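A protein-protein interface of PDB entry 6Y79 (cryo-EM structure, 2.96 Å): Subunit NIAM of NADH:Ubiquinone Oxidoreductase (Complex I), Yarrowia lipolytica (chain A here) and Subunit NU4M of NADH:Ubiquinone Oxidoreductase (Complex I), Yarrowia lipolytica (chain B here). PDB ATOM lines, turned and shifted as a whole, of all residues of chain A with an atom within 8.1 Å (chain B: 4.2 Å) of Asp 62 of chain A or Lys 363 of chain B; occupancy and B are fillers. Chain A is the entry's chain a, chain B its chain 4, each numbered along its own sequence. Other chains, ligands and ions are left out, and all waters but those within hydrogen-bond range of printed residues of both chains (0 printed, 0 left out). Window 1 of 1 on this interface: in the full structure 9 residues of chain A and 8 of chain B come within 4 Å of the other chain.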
ATOM      1  N   PRO A  47     -17.454  30.513  17.216  1.00  0.00           N
ATOM      2  CA  PRO A  47     -16.387  29.510  17.289  1.00  0.00           C
ATOM      3  C   PRO A  47     -15.106  30.086  17.864  1.00  0.00           C
ATOM      4  O   PRO A  47     -14.718  31.216  17.564  1.00  0.00           O
ATOM      5  CB  PRO A  47     -16.205  29.083  15.828  1.00  0.00           C
ATOM      6  CG  PRO A  47     -16.816  30.180  15.025  1.00  0.00           C
ATOM      7  CD  PRO A  47     -17.944  30.694  15.844  1.00  0.00           C
ATOM      8  N   ALA A  48     -14.455  29.296  18.715  1.00  0.00           N
ATOM      9  CA  ALA A  48     -13.266  29.767  19.405  1.00  0.00           C
ATOM     10  C   ALA A  48     -12.049  29.831  18.503  1.00  0.00           C
ATOM     11  O   ALA A  48     -11.059  30.451  18.888  1.00  0.00           O
ATOM     12  CB  ALA A  48     -12.961  28.883  20.610  1.00  0.00           C
ATOM     13  N   GLN A  49     -12.106  29.234  17.317  1.00  0.00           N
ATOM     14  CA  GLN A  49     -11.001  29.291  16.373  1.00  0.00           C
ATOM     15  C   GLN A  49     -11.045  30.543  15.515  1.00  0.00           C
ATOM     16  O   GLN A  49     -10.012  31.181  15.287  1.00  0.00           O
ATOM     17  CB  GLN A  49     -11.026  28.059  15.480  1.00  0.00           C
ATOM     18  CG  GLN A  49      -9.955  28.050  14.428  1.00  0.00           C
ATOM     19  CD  GLN A  49      -9.955  26.772  13.653  1.00  0.00           C
ATOM     20  OE1 GLN A  49     -10.751  25.883  13.924  1.00  0.00           O
ATOM     21  NE2 GLN A  49      -9.054  26.659  12.687  1.00  0.00           N
ATOM     22  N   LYS A  51     -12.014  33.380  16.270  1.00  0.00           N
ATOM     23  CA  LYS A  51     -11.530  34.551  16.976  1.00  0.00           C
ATOM     24  C   LYS A  51     -10.157  34.954  16.453  1.00  0.00           C
ATOM     25  O   LYS A  51      -9.459  34.172  15.798  1.00  0.00           O
ATOM     26  CB  LYS A  51     -11.441  34.268  18.472  1.00  0.00           C
ATOM     27  CG  LYS A  51     -12.770  33.949  19.108  1.00  0.00           C
ATOM     28  CD  LYS A  51     -12.650  33.782  20.599  1.00  0.00           C
ATOM     29  CE  LYS A  51     -14.008  33.525  21.211  1.00  0.00           C
ATOM     30  NZ  LYS A  51     -13.920  33.357  22.687  1.00  0.00           N
ATOM     31  N   TYR A  57      -5.399  36.808  25.171  1.00  0.00           N
ATOM     32  CA  TYR A  57      -6.365  36.181  26.050  1.00  0.00           C
ATOM     33  C   TYR A  57      -5.655  35.717  27.307  1.00  0.00           C
ATOM     34  O   TYR A  57      -4.429  35.739  27.392  1.00  0.00           O
ATOM     35  CB  TYR A  57      -7.025  34.980  25.374  1.00  0.00           C
ATOM     36  CG  TYR A  57      -7.844  35.318  24.175  1.00  0.00           C
ATOM     37  CD1 TYR A  57      -9.142  35.756  24.318  1.00  0.00           C
ATOM     38  CD2 TYR A  57      -7.325  35.183  22.896  1.00  0.00           C
ATOM     39  CE1 TYR A  57      -9.906  36.049  23.239  1.00  0.00           C
ATOM     40  CE2 TYR A  57      -8.087  35.479  21.797  1.00  0.00           C
ATOM     41  CZ  TYR A  57      -9.378  35.913  21.983  1.00  0.00           C
ATOM     42  OH  TYR A  57     -10.169  36.216  20.912  1.00  0.00           O
ATOM     43  N   ASP A  58      -6.438  35.267  28.286  1.00  0.00           N
ATOM     44  CA  ASP A  58      -5.839  34.675  29.478  1.00  0.00           C
ATOM     45  C   ASP A  58      -5.215  33.325  29.152  1.00  0.00           C
ATOM     46  O   ASP A  58      -4.075  33.045  29.539  1.00  0.00           O
ATOM     47  CB  ASP A  58      -6.879  34.568  30.586  1.00  0.00           C
ATOM     48  CG  ASP A  58      -7.337  35.929  31.060  1.00  0.00           C
ATOM     49  OD1 ASP A  58      -6.492  36.675  31.597  1.00  0.00           O
ATOM     50  OD2 ASP A  58      -8.523  36.269  30.890  1.00  0.00           O
ATOM     51  N   ASP A  59      -5.938  32.473  28.428  1.00  0.00           N
ATOM     52  CA  ASP A  59      -5.334  31.319  27.776  1.00  0.00           C
ATOM     53  C   ASP A  59      -5.206  31.617  26.281  1.00  0.00           C
ATOM     54  O   ASP A  59      -6.193  31.869  25.593  1.00  0.00           O
ATOM     55  CB  ASP A  59      -6.082  30.004  28.092  1.00  0.00           C
ATOM     56  CG  ASP A  59      -7.613  30.067  27.924  1.00  0.00           C
ATOM     57  OD1 ASP A  59      -8.139  30.994  27.316  1.00  0.00           O
ATOM     58  OD2 ASP A  59      -8.297  29.163  28.438  1.00  0.00           O
ATOM     59  N   GLN A  60      -3.973  31.663  25.789  1.00  0.00           N
ATOM     60  CA  GLN A  60      -3.769  31.886  24.365  1.00  0.00           C
ATOM     61  C   GLN A  60      -4.223  30.673  23.573  1.00  0.00           C
ATOM     62  O   GLN A  60      -4.649  30.807  22.422  1.00  0.00           O
ATOM     63  CB  GLN A  60      -2.293  32.229  24.082  1.00  0.00           C
ATOM     64  CG  GLN A  60      -2.005  32.677  22.658  1.00  0.00           C
ATOM     65  CD  GLN A  60      -2.788  33.906  22.250  1.00  0.00           C
ATOM     66  OE1 GLN A  60      -3.007  34.816  23.044  1.00  0.00           O
ATOM     67  NE2 GLN A  60      -3.216  33.937  20.996  1.00  0.00           N
ATOM     68  N   GLN A  61      -4.213  29.496  24.200  1.00  0.00           N
ATOM     69  CA  GLN A  61      -4.527  28.266  23.491  1.00  0.00           C
ATOM     70  C   GLN A  61      -6.023  28.094  23.258  1.00  0.00           C
ATOM     71  O   GLN A  61      -6.439  27.775  22.137  1.00  0.00           O
ATOM     72  CB  GLN A  61      -3.969  27.076  24.255  1.00  0.00           C
ATOM     73  CG  GLN A  61      -3.919  25.880  23.390  1.00  0.00           C
ATOM     74  CD  GLN A  61      -3.353  24.663  24.051  1.00  0.00           C
ATOM     75  OE1 GLN A  61      -2.905  24.711  25.183  1.00  0.00           O
ATOM     76  NE2 GLN A  61      -3.388  23.548  23.347  1.00  0.00           N
ATOM     77  N   ASP A  62      -6.843  28.274  24.296  1.00  0.00           N
ATOM     78  CA  ASP A  62      -8.279  28.133  24.116  1.00  0.00           C
ATOM     79  C   ASP A  62      -8.923  29.409  23.603  1.00  0.00           C
ATOM     80  O   ASP A  62     -10.094  29.365  23.209  1.00  0.00           O
ATOM     81  CB  ASP A  62      -8.944  27.699  25.411  1.00  0.00           C
ATOM     82  CG  ASP A  62      -8.317  26.467  26.001  1.00  0.00           C
ATOM     83  OD1 ASP A  62      -8.618  25.343  25.530  1.00  0.00           O
ATOM     84  OD2 ASP A  62      -7.520  26.631  26.938  1.00  0.00           O
ATOM     85  N   ARG A  63      -8.187  30.525  23.606  1.00  0.00           N
ATOM     86  CA  ARG A  63      -8.646  31.847  23.168  1.00  0.00           C
ATOM     87  C   ARG A  63      -9.894  32.276  23.938  1.00  0.00           C
ATOM     88  O   ARG A  63     -10.990  32.404  23.398  1.00  0.00           O
ATOM     89  CB  ARG A  63      -8.895  31.900  21.658  1.00  0.00           C
ATOM     90  CG  ARG A  63      -7.654  31.997  20.786  1.00  0.00           C
ATOM     91  CD  ARG A  63      -8.027  31.411  19.469  1.00  0.00           C
ATOM     92  NE  ARG A  63      -7.397  31.933  18.271  1.00  0.00           N
ATOM     93  CZ  ARG A  63      -7.061  31.159  17.247  1.00  0.00           C
ATOM     94  NH1 ARG A  63      -7.286  29.863  17.302  1.00  0.00           N
ATOM     95  NH2 ARG A  63      -6.510  31.665  16.164  1.00  0.00           N
ATOM     96  N   ARG A  64      -9.690  32.468  25.238  1.00  0.00           N
ATOM     97  CA  ARG A  64     -10.813  32.698  26.130  1.00  0.00           C
ATOM     98  C   ARG A  64     -10.388  33.571  27.304  1.00  0.00           C
ATOM     99  O   ARG A  64      -9.343  33.344  27.909  1.00  0.00           O
ATOM    100  CB  ARG A  64     -11.356  31.356  26.610  1.00  0.00           C
ATOM    101  CG  ARG A  64     -12.585  31.456  27.435  1.00  0.00           C
ATOM    102  CD  ARG A  64     -12.999  30.106  27.926  1.00  0.00           C
ATOM    103  NE  ARG A  64     -14.119  30.242  28.838  1.00  0.00           N
ATOM    104  CZ  ARG A  64     -13.994  30.344  30.152  1.00  0.00           C
ATOM    105  NH1 ARG A  64     -12.797  30.304  30.709  1.00  0.00           N
ATOM    106  NH2 ARG A  64     -15.067  30.476  30.909  1.00  0.00           N
ATOM    107  N   ASN A  65     -11.190  34.576  27.622  1.00  0.00           N
ATOM    108  CA  ASN A  65     -10.912  35.366  28.807  1.00  0.00           C
ATOM    109  C   ASN A  65     -11.494  34.668  30.033  1.00  0.00           C
ATOM    110  O   ASN A  65     -12.358  33.800  29.914  1.00  0.00           O
ATOM    111  CB  ASN A  65     -11.460  36.777  28.646  1.00  0.00           C
ATOM    112  CG  ASN A  65     -10.662  37.585  27.656  1.00  0.00           C
ATOM    113  OD1 ASN A  65      -9.436  37.543  27.655  1.00  0.00           O
ATOM    114  ND2 ASN A  65     -11.351  38.321  26.800  1.00  0.00           N
ATOM    115  N   GLU A  68     -15.610  34.541  31.094  1.00  0.00           N
ATOM    116  CA  GLU A  68     -16.391  34.848  29.923  1.00  0.00           C
ATOM    117  C   GLU A  68     -17.511  33.825  29.856  1.00  0.00           C
ATOM    118  O   GLU A  68     -17.247  32.633  30.056  1.00  0.00           O
ATOM    119  CB  GLU A  68     -15.517  34.786  28.657  1.00  0.00           C
ATOM    120  CG  GLU A  68     -16.128  35.383  27.404  1.00  0.00           C
ATOM    121  CD  GLU A  68     -15.078  35.870  26.416  1.00  0.00           C
ATOM    122  OE1 GLU A  68     -14.341  35.025  25.862  1.00  0.00           O
ATOM    123  OE2 GLU A  68     -14.995  37.095  26.184  1.00  0.00           O
ATOM    124  N   TYR A  77     -18.377  24.740  20.113  1.00  0.00           N
ATOM    125  CA  TYR A  77     -17.737  25.997  19.752  1.00  0.00           C
ATOM    126  C   TYR A  77     -16.433  26.189  20.506  1.00  0.00           C
ATOM    127  O   TYR A  77     -15.950  27.316  20.635  1.00  0.00           O
ATOM    128  CB  TYR A  77     -18.686  27.163  20.008  1.00  0.00           C
ATOM    129  CG  TYR A  77     -19.887  27.106  19.118  1.00  0.00           C
ATOM    130  CD1 TYR A  77     -19.822  27.566  17.815  1.00  0.00           C
ATOM    131  CD2 TYR A  77     -21.076  26.561  19.565  1.00  0.00           C
ATOM    132  CE1 TYR A  77     -20.914  27.503  16.986  1.00  0.00           C
ATOM    133  CE2 TYR A  77     -22.170  26.479  18.744  1.00  0.00           C
ATOM    134  CZ  TYR A  77     -22.087  26.964  17.457  1.00  0.00           C
ATOM    135  OH  TYR A  77     -23.179  26.900  16.630  1.00  0.00           O
ATOM    136  N   ASP A  78     -15.863  25.108  21.010  1.00  0.00           N
ATOM    137  CA  ASP A  78     -14.598  25.171  21.705  1.00  0.00           C
ATOM    138  C   ASP A  78     -13.457  25.044  20.699  1.00  0.00           C
ATOM    139  O   ASP A  78     -13.652  24.825  19.505  1.00  0.00           O
ATOM    140  CB  ASP A  78     -14.535  24.075  22.773  1.00  0.00           C
ATOM    141  CG  ASP A  78     -13.454  24.316  23.823  1.00  0.00           C
ATOM    142  OD1 ASP A  78     -12.827  25.397  23.792  1.00  0.00           O
ATOM    143  OD2 ASP A  78     -13.225  23.419  24.658  1.00  0.00           O
ATOM    144  N   MET A  79     -12.251  25.238  21.205  1.00  0.00           N
ATOM    145  CA  MET A  79     -11.046  24.982  20.449  1.00  0.00           C
ATOM    146  C   MET A  79     -10.862  23.502  20.142  1.00  0.00           C
ATOM    147  O   MET A  79     -10.271  23.151  19.114  1.00  0.00           O
ATOM    148  CB  MET A  79      -9.887  25.527  21.258  1.00  0.00           C
ATOM    149  CG  MET A  79      -8.651  25.611  20.512  1.00  0.00           C
ATOM    150  SD  MET A  79      -8.810  26.328  18.892  1.00  0.00           S
ATOM    151  CE  MET A  79      -9.031  27.971  19.459  1.00  0.00           C
ATOM    152  N   TRP A  80     -11.358  22.626  21.010  1.00  0.00           N
ATOM    153  CA  TRP A  80     -11.259  21.183  20.830  1.00  0.00           C
ATOM    154  C   TRP A  80     -12.382  20.604  19.985  1.00  0.00           C
ATOM    155  O   TRP A  80     -12.501  19.385  19.905  1.00  0.00           O
ATOM    156  CB  TRP A  80     -11.217  20.496  22.198  1.00  0.00           C
ATOM    157  CG  TRP A  80      -9.965  20.730  22.943  1.00  0.00           C
ATOM    158  CD1 TRP A  80      -9.726  21.711  23.851  1.00  0.00           C
ATOM    159  CD2 TRP A  80      -8.759  19.976  22.838  1.00  0.00           C
ATOM    160  NE1 TRP A  80      -8.446  21.612  24.326  1.00  0.00           N
ATOM    161  CE2 TRP A  80      -7.829  20.553  23.716  1.00  0.00           C
ATOM    162  CE3 TRP A  80      -8.375  18.867  22.085  1.00  0.00           C
ATOM    163  CZ2 TRP A  80      -6.544  20.054  23.870  1.00  0.00           C
ATOM    164  CZ3 TRP A  80      -7.100  18.376  22.234  1.00  0.00           C
ATOM    165  CH2 TRP A  80      -6.199  18.968  23.118  1.00  0.00           C
ATOM    166  N   TYR B 361     -11.693  22.193  33.150  1.00  0.00           N
ATOM    167  CA  TYR B 361     -10.544  22.667  33.901  1.00  0.00           C
ATOM    168  C   TYR B 361      -9.273  21.915  33.577  1.00  0.00           C
ATOM    169  O   TYR B 361      -8.188  22.432  33.841  1.00  0.00           O
ATOM    170  CB  TYR B 361     -10.778  22.539  35.396  1.00  0.00           C
ATOM    171  CG  TYR B 361     -11.859  23.414  35.930  1.00  0.00           C
ATOM    172  CD1 TYR B 361     -11.642  24.760  36.160  1.00  0.00           C
ATOM    173  CD2 TYR B 361     -13.097  22.891  36.220  1.00  0.00           C
ATOM    174  CE1 TYR B 361     -12.634  25.557  36.660  1.00  0.00           C
ATOM    175  CE2 TYR B 361     -14.086  23.673  36.721  1.00  0.00           C
ATOM    176  CZ  TYR B 361     -13.856  25.004  36.937  1.00  0.00           C
ATOM    177  OH  TYR B 361     -14.865  25.780  37.437  1.00  0.00           O
ATOM    178  N   TYR B 362      -9.376  20.716  33.037  1.00  0.00           N
ATOM    179  CA  TYR B 362      -8.253  19.796  32.948  1.00  0.00           C
ATOM    180  C   TYR B 362      -7.694  19.823  31.532  1.00  0.00           C
ATOM    181  O   TYR B 362      -8.401  19.509  30.572  1.00  0.00           O
ATOM    182  CB  TYR B 362      -8.706  18.395  33.334  1.00  0.00           C
ATOM    183  CG  TYR B 362      -9.095  18.240  34.776  1.00  0.00           C
ATOM    184  CD1 TYR B 362      -8.319  18.765  35.784  1.00  0.00           C
ATOM    185  CD2 TYR B 362     -10.262  17.604  35.123  1.00  0.00           C
ATOM    186  CE1 TYR B 362      -8.679  18.630  37.105  1.00  0.00           C
ATOM    187  CE2 TYR B 362     -10.632  17.461  36.435  1.00  0.00           C
ATOM    188  CZ  TYR B 362      -9.837  17.976  37.421  1.00  0.00           C
ATOM    189  OH  TYR B 362     -10.205  17.842  38.730  1.00  0.00           O
ATOM    190  N   LYS B 363      -6.426  20.195  31.407  1.00  0.00           N
ATOM    191  CA  LYS B 363      -5.758  20.273  30.119  1.00  0.00           C
ATOM    192  C   LYS B 363      -4.260  20.200  30.354  1.00  0.00           C
ATOM    193  O   LYS B 363      -3.746  20.841  31.271  1.00  0.00           O
ATOM    194  CB  LYS B 363      -6.115  21.566  29.382  1.00  0.00           C
ATOM    195  CG  LYS B 363      -5.549  21.657  27.985  1.00  0.00           C
ATOM    196  CD  LYS B 363      -5.991  22.917  27.281  1.00  0.00           C
ATOM    197  CE  LYS B 363      -5.374  24.126  27.922  1.00  0.00           C
ATOM    198  NZ  LYS B 363      -5.498  25.318  27.060  1.00  0.00           N
ATOM    199  N   GLY B 364      -3.574  19.412  29.534  1.00  0.00           N
ATOM    200  CA  GLY B 364      -2.127  19.381  29.543  1.00  0.00           C
ATOM    201  C   GLY B 364      -1.524  18.799  30.795  1.00  0.00           C
ATOM    202  O   GLY B 364      -0.610  19.381  31.380  1.00  0.00           O
ATOM    203  N   LEU B 365      -2.025  17.646  31.217  1.00  0.00           N
ATOM    204  CA  LEU B 365      -1.564  17.023  32.448  1.00  0.00           C
ATOM    205  C   LEU B 365      -0.222  16.308  32.309  1.00  0.00           C
ATOM    206  O   LEU B 365       0.291  15.834  33.322  1.00  0.00           O
ATOM    207  CB  LEU B 365      -2.627  16.038  32.956  1.00  0.00           C
ATOM    208  CG  LEU B 365      -3.753  16.484  33.895  1.00  0.00           C
ATOM    209  CD1 LEU B 365      -4.801  17.304  33.174  1.00  0.00           C
ATOM    210  CD2 LEU B 365      -4.393  15.265  34.503  1.00  0.00           C
ATOM    211  N   LYS B 430      -7.633  15.221  25.393  1.00  0.00           N
ATOM    212  CA  LYS B 430      -7.909  16.465  26.100  1.00  0.00           C
ATOM    213  C   LYS B 430      -7.185  16.507  27.437  1.00  0.00           C
ATOM    214  O   LYS B 430      -6.634  17.544  27.818  1.00  0.00           O
ATOM    215  CB  LYS B 430      -9.414  16.622  26.301  1.00  0.00           C
ATOM    216  CG  LYS B 430      -9.822  17.795  27.159  1.00  0.00           C
ATOM    217  CD  LYS B 430      -9.524  19.102  26.468  1.00  0.00           C
ATOM    218  CE  LYS B 430     -10.077  20.290  27.236  1.00  0.00           C
ATOM    219  NZ  LYS B 430     -11.557  20.407  27.107  1.00  0.00           N
ATOM    220  N   LEU B 431      -7.170  15.385  28.161  1.00  0.00           N
ATOM    221  CA  LEU B 431      -6.498  15.362  29.456  1.00  0.00           C
ATOM    222  C   LEU B 431      -4.988  15.422  29.307  1.00  0.00           C
ATOM    223  O   LEU B 431      -4.314  16.108  30.080  1.00  0.00           O
ATOM    224  CB  LEU B 431      -6.882  14.110  30.239  1.00  0.00           C
ATOM    225  CG  LEU B 431      -8.300  13.994  30.783  1.00  0.00           C
ATOM    226  CD1 LEU B 431      -8.460  12.661  31.463  1.00  0.00           C
ATOM    227  CD2 LEU B 431      -8.585  15.104  31.738  1.00  0.00           C
ATOM    228  N   GLY B 433      -3.093  16.242  26.353  1.00  0.00           N
ATOM    229  CA  GLY B 433      -2.561  17.237  25.450  1.00  0.00           C
ATOM    230  C   GLY B 433      -2.844  18.676  25.853  1.00  0.00           C
ATOM    231  O   GLY B 433      -3.706  18.973  26.672  1.00  0.00           O
ATOM    232  N   ILE B 435      -1.158  22.934  26.401  1.00  0.00           N
ATOM    233  CA  ILE B 435      -0.428  23.634  27.451  1.00  0.00           C
ATOM    234  C   ILE B 435      -1.139  23.344  28.763  1.00  0.00           C
ATOM    235  O   ILE B 435      -2.354  23.118  28.782  1.00  0.00           O
ATOM    236  CB  ILE B 435      -0.349  25.142  27.135  1.00  0.00           C
ATOM    237  CG1 ILE B 435       0.343  25.361  25.792  1.00  0.00           C
ATOM    238  CG2 ILE B 435       0.401  25.937  28.181  1.00  0.00           C
ATOM    239  CD1 ILE B 435       0.225  26.768  25.273  1.00  0.00           C
ATOM    240  N   SER B 436      -0.364  23.260  29.847  1.00  0.00           N
ATOM    241  CA  SER B 436      -0.893  23.062  31.191  1.00  0.00           C
ATOM    242  C   SER B 436      -1.973  24.078  31.537  1.00  0.00           C
ATOM    243  O   SER B 436      -1.955  25.219  31.070  1.00  0.00           O
ATOM    244  CB  SER B 436       0.239  23.157  32.205  1.00  0.00           C
ATOM    245  OG  SER B 436      -0.260  23.035  33.520  1.00  0.00           O
ATOM    246  N   SER B 437      -2.931  23.637  32.342  1.00  0.00           N
ATOM    247  CA  SER B 437      -4.128  24.419  32.599  1.00  0.00           C
ATOM    248  C   SER B 437      -3.817  25.621  33.476  1.00  0.00           C
ATOM    249  O   SER B 437      -3.021  25.541  34.413  1.00  0.00           O
ATOM    250  CB  SER B 437      -5.182  23.546  33.266  1.00  0.00           C
ATOM    251  OG  SER B 437      -6.367  24.270  33.527  1.00  0.00           O
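The side-chain amino group (NZ) of Lys 363 of chain B lies within salt-bridge range of the side-chain carboxylate (OD2) of Asp 62 of chain A (2.4 Å).
N of Ile 435 of chain B is in hydrogen-bond range of OE1 of Gln 61 of chain A (2.8 Å).
NZ of Lys 363 of chain B lies within hydrogen-bond range of OE1 of Gln 61 of chain A.
The backbone carbonyl oxygen (O) of Lys 363 of chain B lies within hydrogen-bond range of the backbone NH (N) of Ser 437 of chain B (3.1 Å).
Lys 430 of chain B touches Trp 80 of chain A.
Asp 58 of chain A touches none of the printed residues of chain B.
Printed residues of chain B within 4 Å of Gln 61 of chain A: Lys 363 and Ile 435.
Asp 62 of chain A touches one residue of chain B.
Arg 64 of chain A touches none of the printed residues of chain B.
Printed residues of chain B within 4 Å of Trp 80 of chain A: Lys 430 (3.5 Å).
Of the printed residues of chain A, Lys 363 of chain B touches Gln 61 (3.3 Å) and Asp 62 (2.4 Å).
Gly 364 of chain B touches none of the printed residues of chain A.
Of the printed residues of chain A, Lys 430 of chain B touches Trp 80 (3.5 Å).
Of the printed residues of chain A, Ile 435 of chain B touches Gln 61.
The nearest printed residue of chain B that does not touch Asp 62 of chain A is Lys 430 of chain B (5.5 Å).
Hydrophobic or aromatic side chains of chain B that line the printed part of chain A: Ile 435.
Of the 18 printed residues of chain A, 3 touch a printed residue of chain B.
Among the printed residues, 4 pairs touch across the chains.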
